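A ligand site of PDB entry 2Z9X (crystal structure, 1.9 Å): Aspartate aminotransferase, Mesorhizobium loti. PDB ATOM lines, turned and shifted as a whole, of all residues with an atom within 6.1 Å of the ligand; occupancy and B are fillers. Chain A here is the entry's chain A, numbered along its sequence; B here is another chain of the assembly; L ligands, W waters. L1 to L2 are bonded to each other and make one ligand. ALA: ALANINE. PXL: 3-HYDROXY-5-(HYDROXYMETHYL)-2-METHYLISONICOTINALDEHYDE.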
ATOM      1  N   ALA A  15      18.095 -25.230  -0.886  1.00  0.00           N
ATOM      2  CA  ALA A  15      17.874 -25.593  -2.285  1.00  0.00           C
ATOM      3  C   ALA A  15      18.908 -24.977  -3.234  1.00  0.00           C
ATOM      4  O   ALA A  15      18.683 -24.892  -4.424  1.00  0.00           O
ATOM      5  CB  ALA A  15      16.427 -25.189  -2.705  1.00  0.00           C
ATOM      6  N   GLY A  16      20.042 -24.525  -2.685  1.00  0.00           N
ATOM      7  CA  GLY A  16      21.148 -24.029  -3.516  1.00  0.00           C
ATOM      8  C   GLY A  16      21.656 -22.699  -2.973  1.00  0.00           C
ATOM      9  O   GLY A  16      20.931 -21.715  -2.950  1.00  0.00           O
ATOM     10  N   PRO A  17      22.917 -22.668  -2.493  1.00  0.00           N
ATOM     11  CA  PRO A  17      23.847 -23.786  -2.394  1.00  0.00           C
ATOM     12  C   PRO A  17      23.338 -24.856  -1.428  1.00  0.00           C
ATOM     13  O   PRO A  17      22.369 -24.616  -0.694  1.00  0.00           O
ATOM     14  CB  PRO A  17      25.132 -23.153  -1.810  1.00  0.00           C
ATOM     15  CG  PRO A  17      24.775 -21.836  -1.311  1.00  0.00           C
ATOM     16  CD  PRO A  17      23.486 -21.408  -1.961  1.00  0.00           C
ATOM     17  N   GLU A  67      30.143 -20.240 -11.658  1.00  0.00           N
ATOM     18  CA  GLU A  67      28.907 -20.961 -11.333  1.00  0.00           C
ATOM     19  C   GLU A  67      27.884 -20.784 -12.479  1.00  0.00           C
ATOM     20  O   GLU A  67      28.066 -19.920 -13.367  1.00  0.00           O
ATOM     21  CB  GLU A  67      28.387 -20.592  -9.929  1.00  0.00           C
ATOM     22  CG  GLU A  67      27.513 -19.354  -9.815  1.00  0.00           C
ATOM     23  CD  GLU A  67      26.021 -19.704  -9.783  1.00  0.00           C
ATOM     24  OE1 GLU A  67      25.269 -19.061 -10.511  1.00  0.00           O
ATOM     25  OE2 GLU A  67      25.576 -20.568  -9.009  1.00  0.00           O
ATOM     26  N   PRO A  68      26.845 -21.626 -12.512  1.00  0.00           N
ATOM     27  CA  PRO A  68      25.982 -21.707 -13.702  1.00  0.00           C
ATOM     28  C   PRO A  68      25.327 -20.439 -14.285  1.00  0.00           C
ATOM     29  O   PRO A  68      24.959 -20.488 -15.456  1.00  0.00           O
ATOM     30  CB  PRO A  68      24.899 -22.713 -13.293  1.00  0.00           C
ATOM     31  CG  PRO A  68      25.640 -23.660 -12.408  1.00  0.00           C
ATOM     32  CD  PRO A  68      26.461 -22.662 -11.525  1.00  0.00           C
ATOM     33  N   VAL A  69      25.195 -19.344 -13.543  1.00  0.00           N
ATOM     34  CA  VAL A  69      24.720 -18.090 -14.204  1.00  0.00           C
ATOM     35  C   VAL A  69      25.680 -17.710 -15.329  1.00  0.00           C
ATOM     36  O   VAL A  69      25.270 -17.064 -16.292  1.00  0.00           O
ATOM     37  CB  VAL A  69      24.517 -16.877 -13.267  1.00  0.00           C
ATOM     38  CG1 VAL A  69      23.347 -17.106 -12.316  1.00  0.00           C
ATOM     39  CG2 VAL A  69      25.826 -16.512 -12.517  1.00  0.00           C
ATOM     40  N   LEU A  72      24.478 -19.751 -18.389  1.00  0.00           N
ATOM     41  CA  LEU A  72      23.239 -19.181 -18.915  1.00  0.00           C
ATOM     42  C   LEU A  72      23.480 -17.914 -19.722  1.00  0.00           C
ATOM     43  O   LEU A  72      22.982 -17.780 -20.842  1.00  0.00           O
ATOM     44  CB  LEU A  72      22.228 -18.930 -17.789  1.00  0.00           C
ATOM     45  CG  LEU A  72      21.767 -20.173 -17.019  1.00  0.00           C
ATOM     46  CD1 LEU A  72      20.960 -19.731 -15.809  1.00  0.00           C
ATOM     47  CD2 LEU A  72      20.994 -21.190 -17.918  1.00  0.00           C
ATOM     48  N   TYR A  94      13.668 -17.958 -12.635  1.00  0.00           N
ATOM     49  CA  TYR A  94      14.768 -18.187 -13.603  1.00  0.00           C
ATOM     50  C   TYR A  94      14.323 -18.156 -15.064  1.00  0.00           C
ATOM     51  O   TYR A  94      15.009 -17.606 -15.901  1.00  0.00           O
ATOM     52  CB  TYR A  94      15.591 -19.443 -13.279  1.00  0.00           C
ATOM     53  CG  TYR A  94      16.514 -19.150 -12.123  1.00  0.00           C
ATOM     54  CD1 TYR A  94      17.797 -18.623 -12.347  1.00  0.00           C
ATOM     55  CD2 TYR A  94      16.084 -19.356 -10.822  1.00  0.00           C
ATOM     56  CE1 TYR A  94      18.640 -18.317 -11.252  1.00  0.00           C
ATOM     57  CE2 TYR A  94      16.896 -19.068  -9.747  1.00  0.00           C
ATOM     58  CZ  TYR A  94      18.159 -18.538  -9.962  1.00  0.00           C
ATOM     59  OH  TYR A  94      18.948 -18.254  -8.857  1.00  0.00           O
ATOM     60  N   CYS A 141      13.464 -23.408 -18.555  1.00  0.00           N
ATOM     61  CA  CYS A 141      14.075 -23.835 -17.304  1.00  0.00           C
ATOM     62  C   CYS A 141      13.383 -25.155 -16.865  1.00  0.00           C
ATOM     63  O   CYS A 141      12.162 -25.195 -16.787  1.00  0.00           O
ATOM     64  CB  CYS A 141      13.880 -22.746 -16.246  1.00  0.00           C
ATOM     65  SG  CYS A 141      14.645 -23.097 -14.644  1.00  0.00           S
ATOM     66  N   HIS A 143      13.872 -27.108 -13.742  1.00  0.00           N
ATOM     67  CA  HIS A 143      13.404 -26.927 -12.385  1.00  0.00           C
ATOM     68  C   HIS A 143      13.592 -25.459 -12.022  1.00  0.00           C
ATOM     69  O   HIS A 143      14.727 -24.998 -11.808  1.00  0.00           O
ATOM     70  CB  HIS A 143      14.170 -27.895 -11.457  1.00  0.00           C
ATOM     71  CG  HIS A 143      13.911 -27.737  -9.977  1.00  0.00           C
ATOM     72  ND1 HIS A 143      12.741 -27.208  -9.447  1.00  0.00           N
ATOM     73  CD2 HIS A 143      14.676 -28.085  -8.921  1.00  0.00           C
ATOM     74  CE1 HIS A 143      12.827 -27.224  -8.127  1.00  0.00           C
ATOM     75  NE2 HIS A 143      13.979 -27.755  -7.788  1.00  0.00           N
ATOM     76  N   ASP A 144      12.492 -24.706 -11.985  1.00  0.00           N
ATOM     77  CA  ASP A 144      12.603 -23.288 -11.630  1.00  0.00           C
ATOM     78  C   ASP A 144      12.596 -23.204 -10.125  1.00  0.00           C
ATOM     79  O   ASP A 144      11.543 -23.074  -9.492  1.00  0.00           O
ATOM     80  CB  ASP A 144      11.510 -22.451 -12.276  1.00  0.00           C
ATOM     81  CG  ASP A 144      11.916 -20.981 -12.456  1.00  0.00           C
ATOM     82  OD1 ASP A 144      12.490 -20.422 -11.495  1.00  0.00           O
ATOM     83  OD2 ASP A 144      11.689 -20.406 -13.550  1.00  0.00           O
ATOM     84  N   THR A 145      13.798 -23.279  -9.559  1.00  0.00           N
ATOM     85  CA  THR A 145      14.005 -23.678  -8.178  1.00  0.00           C
ATOM     86  C   THR A 145      13.183 -22.856  -7.146  1.00  0.00           C
ATOM     87  O   THR A 145      12.621 -23.426  -6.212  1.00  0.00           O
ATOM     88  CB  THR A 145      15.528 -23.747  -7.838  1.00  0.00           C
ATOM     89  OG1 THR A 145      16.266 -24.182  -8.994  1.00  0.00           O
ATOM     90  CG2 THR A 145      15.763 -24.730  -6.684  1.00  0.00           C
ATOM     91  N   PRO A 146      13.146 -21.515  -7.282  1.00  0.00           N
ATOM     92  CA  PRO A 146      12.365 -20.687  -6.326  1.00  0.00           C
ATOM     93  C   PRO A 146      10.873 -21.024  -6.255  1.00  0.00           C
ATOM     94  O   PRO A 146      10.184 -20.544  -5.362  1.00  0.00           O
ATOM     95  CB  PRO A 146      12.594 -19.255  -6.845  1.00  0.00           C
ATOM     96  CG  PRO A 146      13.942 -19.331  -7.571  1.00  0.00           C
ATOM     97  CD  PRO A 146      13.912 -20.684  -8.236  1.00  0.00           C
ATOM     98  N   ASP A 170      18.031 -24.761 -18.970  1.00  0.00           N
ATOM     99  CA  ASP A 170      18.606 -24.617 -17.638  1.00  0.00           C
ATOM    100  C   ASP A 170      18.182 -25.863 -16.827  1.00  0.00           C
ATOM    101  O   ASP A 170      17.016 -25.977 -16.420  1.00  0.00           O
ATOM    102  CB  ASP A 170      18.042 -23.351 -16.972  1.00  0.00           C
ATOM    103  CG  ASP A 170      18.461 -23.197 -15.517  1.00  0.00           C
ATOM    104  OD1 ASP A 170      18.400 -22.054 -15.000  1.00  0.00           O
ATOM    105  OD2 ASP A 170      18.813 -24.217 -14.885  1.00  0.00           O
ATOM    106  N   VAL A 172      20.108 -26.767 -14.070  1.00  0.00           N
ATOM    107  CA  VAL A 172      21.041 -26.586 -12.949  1.00  0.00           C
ATOM    108  C   VAL A 172      20.602 -27.330 -11.686  1.00  0.00           C
ATOM    109  O   VAL A 172      21.431 -27.925 -10.979  1.00  0.00           O
ATOM    110  CB  VAL A 172      21.233 -25.086 -12.655  1.00  0.00           C
ATOM    111  CG1 VAL A 172      21.945 -24.861 -11.291  1.00  0.00           C
ATOM    112  CG2 VAL A 172      21.989 -24.427 -13.799  1.00  0.00           C
ATOM    113  N   SER A 173      19.294 -27.289 -11.400  1.00  0.00           N
ATOM    114  CA  SER A 173      18.762 -27.857 -10.157  1.00  0.00           C
ATOM    115  C   SER A 173      17.978 -29.153 -10.342  1.00  0.00           C
ATOM    116  O   SER A 173      17.241 -29.539  -9.440  1.00  0.00           O
ATOM    117  CB  SER A 173      17.905 -26.827  -9.437  1.00  0.00           C
ATOM    118  OG  SER A 173      16.857 -26.322 -10.256  1.00  0.00           O
ATOM    119  N   LYS A 196      24.120 -28.615  -6.829  1.00  0.00           N
ATOM    120  CA  LYS A 196      22.798 -29.006  -6.389  1.00  0.00           C
ATOM    121  C   LYS A 196      22.790 -30.523  -6.163  1.00  0.00           C
ATOM    122  O   LYS A 196      23.349 -30.999  -5.175  1.00  0.00           O
ATOM    123  CB  LYS A 196      21.728 -28.528  -7.390  1.00  0.00           C
ATOM    124  CG  LYS A 196      21.405 -27.025  -7.229  1.00  0.00           C
ATOM    125  CD  LYS A 196      22.537 -26.143  -7.805  1.00  0.00           C
ATOM    126  CE  LYS A 196      22.279 -24.652  -7.550  1.00  0.00           C
ATOM    127  NZ  LYS A 196      23.403 -23.805  -8.073  1.00  0.00           N
ATOM    128  N   SER A 332      15.707 -22.857   2.776  1.00  0.00           N
ATOM    129  CA  SER A 332      15.831 -21.767   1.818  1.00  0.00           C
ATOM    130  C   SER A 332      14.594 -20.862   1.825  1.00  0.00           C
ATOM    131  O   SER A 332      13.448 -21.316   2.005  1.00  0.00           O
ATOM    132  CB  SER A 332      16.037 -22.297   0.406  1.00  0.00           C
ATOM    133  OG  SER A 332      17.372 -22.711   0.190  1.00  0.00           O
ATOM    134  N   SER A 333      14.847 -19.578   1.593  1.00  0.00           N
ATOM    135  CA  SER A 333      13.796 -18.626   1.298  1.00  0.00           C
ATOM    136  C   SER A 333      13.372 -18.846  -0.146  1.00  0.00           C
ATOM    137  O   SER A 333      14.001 -19.640  -0.876  1.00  0.00           O
ATOM    138  CB  SER A 333      14.332 -17.199   1.467  1.00  0.00           C
ATOM    139  OG  SER A 333      15.269 -16.869   0.456  1.00  0.00           O
ATOM    140  N   GLY A 334      12.297 -18.167  -0.567  1.00  0.00           N
ATOM    141  CA  GLY A 334      12.016 -18.007  -1.989  1.00  0.00           C
ATOM    142  C   GLY A 334      13.021 -17.057  -2.618  1.00  0.00           C
ATOM    143  O   GLY A 334      14.041 -16.713  -2.008  1.00  0.00           O
ATOM    144  N   ARG A 335      12.721 -16.613  -3.836  1.00  0.00           N
ATOM    145  CA  ARG A 335      13.588 -15.683  -4.579  1.00  0.00           C
ATOM    146  C   ARG A 335      12.676 -14.830  -5.456  1.00  0.00           C
ATOM    147  O   ARG A 335      11.687 -15.321  -5.987  1.00  0.00           O
ATOM    148  CB  ARG A 335      14.591 -16.473  -5.429  1.00  0.00           C
ATOM    149  CG  ARG A 335      15.557 -15.613  -6.210  1.00  0.00           C
ATOM    150  CD  ARG A 335      16.613 -16.395  -6.946  1.00  0.00           C
ATOM    151  NE  ARG A 335      17.505 -15.458  -7.635  1.00  0.00           N
ATOM    152  CZ  ARG A 335      18.674 -15.049  -7.148  1.00  0.00           C
ATOM    153  NH1 ARG A 335      19.117 -15.523  -5.987  1.00  0.00           N
ATOM    154  NH2 ARG A 335      19.415 -14.170  -7.818  1.00  0.00           N
ATOM    155  N   ARG A 344      11.504 -23.134   1.051  1.00  0.00           N
ATOM    156  CA  ARG A 344      12.020 -24.287   0.281  1.00  0.00           C
ATOM    157  C   ARG A 344      12.840 -25.230   1.132  1.00  0.00           C
ATOM    158  O   ARG A 344      13.723 -24.822   1.909  1.00  0.00           O
ATOM    159  CB  ARG A 344      12.837 -23.830  -0.939  1.00  0.00           C
ATOM    160  CG  ARG A 344      12.006 -23.152  -2.024  1.00  0.00           C
ATOM    161  CD  ARG A 344      12.879 -22.699  -3.181  1.00  0.00           C
ATOM    162  NE  ARG A 344      13.759 -21.563  -2.852  1.00  0.00           N
ATOM    163  CZ  ARG A 344      14.789 -21.152  -3.599  1.00  0.00           C
ATOM    164  NH1 ARG A 344      15.153 -21.823  -4.704  1.00  0.00           N
ATOM    165  NH2 ARG A 344      15.481 -20.093  -3.228  1.00  0.00           N
ATOM    166  N   TYR B  34      24.598 -22.773   3.287  1.00  0.00           N
ATOM    167  CA  TYR B  34      23.700 -21.908   2.513  1.00  0.00           C
ATOM    168  C   TYR B  34      24.263 -20.490   2.569  1.00  0.00           C
ATOM    169  O   TYR B  34      24.663 -20.033   3.656  1.00  0.00           O
ATOM    170  CB  TYR B  34      22.354 -21.905   3.215  1.00  0.00           C
ATOM    171  CG  TYR B  34      21.202 -21.130   2.572  1.00  0.00           C
ATOM    172  CD1 TYR B  34      20.290 -20.453   3.391  1.00  0.00           C
ATOM    173  CD2 TYR B  34      20.968 -21.163   1.184  1.00  0.00           C
ATOM    174  CE1 TYR B  34      19.196 -19.809   2.861  1.00  0.00           C
ATOM    175  CE2 TYR B  34      19.863 -20.459   0.629  1.00  0.00           C
ATOM    176  CZ  TYR B  34      18.992 -19.808   1.495  1.00  0.00           C
ATOM    177  OH  TYR B  34      17.907 -19.124   1.026  1.00  0.00           O
ATOM    178  N   ASP B  35      24.257 -19.775   1.452  1.00  0.00           N
ATOM    179  CA  ASP B  35      24.878 -18.427   1.443  1.00  0.00           C
ATOM    180  C   ASP B  35      24.088 -17.386   2.209  1.00  0.00           C
ATOM    181  O   ASP B  35      24.643 -16.339   2.609  1.00  0.00           O
ATOM    182  CB  ASP B  35      25.257 -17.942   0.021  1.00  0.00           C
ATOM    183  CG  ASP B  35      24.108 -18.034  -0.985  1.00  0.00           C
ATOM    184  OD1 ASP B  35      23.073 -18.640  -0.685  1.00  0.00           O
ATOM    185  OD2 ASP B  35      24.263 -17.472  -2.094  1.00  0.00           O
ATOM    186  N   THR B 247      25.263 -16.813  -6.729  1.00  0.00           N
ATOM    187  CA  THR B 247      25.824 -17.615  -5.635  1.00  0.00           C
ATOM    188  C   THR B 247      27.387 -17.501  -5.542  1.00  0.00           C
ATOM    189  O   THR B 247      28.100 -17.802  -6.515  1.00  0.00           O
ATOM    190  CB  THR B 247      25.344 -19.081  -5.732  1.00  0.00           C
ATOM    191  OG1 THR B 247      23.910 -19.101  -5.861  1.00  0.00           O
ATOM    192  CG2 THR B 247      25.780 -19.895  -4.514  1.00  0.00           C
HETATM  193  N   ALA L   1      19.351 -20.681  -7.711  1.00  0.00           N
HETATM  194  CA  ALA L   1      19.495 -20.512  -6.243  1.00  0.00           C
HETATM  195  C   ALA L   1      18.088 -20.412  -5.615  1.00  0.00           C
HETATM  196  O   ALA L   1      17.154 -20.979  -6.258  1.00  0.00           O
HETATM  197  CB  ALA L   1      20.356 -19.237  -5.977  1.00  0.00           C
HETATM  198  OXT ALA L   1      17.958 -19.847  -4.509  1.00  0.00           O
HETATM  199  OP4 PXL L   2      23.180 -21.466  -9.982  1.00  0.00           O
HETATM  200  C5A PXL L   2      22.373 -20.524 -10.702  1.00  0.00           C
HETATM  201  C5  PXL L   2      20.980 -21.170 -10.881  1.00  0.00           C
HETATM  202  C6  PXL L   2      20.531 -21.367 -12.187  1.00  0.00           C
HETATM  203  N1  PXL L   2      19.359 -21.924 -12.448  1.00  0.00           N
HETATM  204  C2  PXL L   2      18.532 -22.300 -11.482  1.00  0.00           C
HETATM  205  C3  PXL L   2      18.939 -22.150 -10.151  1.00  0.00           C
HETATM  206  C4  PXL L   2      20.160 -21.557  -9.817  1.00  0.00           C
HETATM  207  C4A PXL L   2      20.510 -21.381  -8.335  1.00  0.00           C
HETATM  208  O3  PXL L   2      18.158 -22.522  -9.140  1.00  0.00           O
HETATM  209  C2A PXL L   2      17.182 -22.943 -11.864  1.00  0.00           C
HETATM  210  O   HOH W   1      23.497 -18.242  -8.487  1.00  0.00           O
HETATM  211  O   HOH W   2      22.889 -21.793  -5.892  1.00  0.00           O
HETATM  212  O   HOH W   3      22.732 -17.554  -4.036  1.00  0.00           O
HETATM  213  O   HOH W   4      19.330 -23.929  -6.968  1.00  0.00           O
HETATM  214  O   HOH W   5      18.263 -21.790  -2.147  1.00  0.00           O
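An oxygen (O3) of PXL L2 lies within hydrogen-bond range of the side-chain hydroxyl (OG1) of Thr 145 (2.5 Å). An oxygen (O) of ALA L1 lies within salt-bridge range of the guanidinium group (NH1) of Arg 344, at 2.7 Å. OE2 of Glu 67 lies within hydrogen-bond range of OP4 of PXL L2 (2.7 Å). N of ALA L1 sits at hydrogen-bond distance from OH of Tyr 94 (2.7 Å). The side-chain amino group (NZ) of Lys 196 lies within hydrogen-bond range of an oxygen (OP4) of PXL L2 (3.0 Å). OD1 of Asp 170 sits at hydrogen-bond distance from N1 of PXL L2, 2.7 Å away.
The side-chain hydroxyl (OG1) of Thr 145 sits at hydrogen-bond distance from the backbone carbonyl oxygen (O) of His 143, at 3.3 Å. The side-chain sulfur (SG) of Cys 141 sits close to the backbone NH (N) of Asp 144. The backbone NH (N) of Arg 344 sits at hydrogen-bond distance from the backbone carbonyl oxygen (O) of Ser 332 (2.8 Å). O of His 143 lies within hydrogen-bond range of SG of Cys 141, 3.4 Å away. O of Thr 145 sits close to NH1 of Arg 344. OH of Tyr 94 is in hydrogen-bond range of NE of Arg 335 (3.4 Å). The backbone NH of Tyr 94 sits at hydrogen-bond distance from the side-chain carboxylate of Asp 144 (3.0 Å). The backbone NH of Val 69 sits at hydrogen-bond distance from the side-chain carboxylate of Glu 67 (3.0 Å).
Merely in contact with the ligand: Gly 16, Pro 68, Val 69, Leu 72, Cys 141, His 143, Pro 146, Val 172, Ser 173, Arg 335 and Thr 247 of chain B. Hydrophobic or aromatic side chains that line the ligand: Pro 68, Val 69, Leu 72, Tyr 94, Pro 146 and Val 172. Along chain A the residues within 4 Å of the ligand span positions 16 to 344. The nearest printed residue that does not touch the ligand is Ala 15 (4.6 Å).
Water W4 bridges the backbone carbonyl oxygen (O) of Ala 15 (2.8 Å) and an oxygen (O3) of PXL L2 (2.8 Å). Water W5 lies within hydrogen-bond range of the side-chain hydroxyl (OG) of Ser 332 (2.7 Å), the backbone carbonyl oxygen (O) of Gly 16 (2.8 Å), an oxygen (OXT) of ALA L1 (3.1 Å) and the guanidinium group (NH2) of Arg 344 (3.4 Å). Water W1 lies within hydrogen-bond range of the side-chain hydroxyl (OG1) of Thr 247 of chain B (2.8 Å) and the side-chain carboxylate (OE1) of Glu 67 (2.8 Å). Water W2 bridges the side-chain hydroxyl (OG1) of Thr 247 of chain B (2.9 Å) and the side-chain amino group (NZ) of Lys 196 (3.0 Å). Water W3 bridges OD2 of Asp 35 of chain B (2.5 Å) and OG1 of Thr 247 of chain B (2.7 Å).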
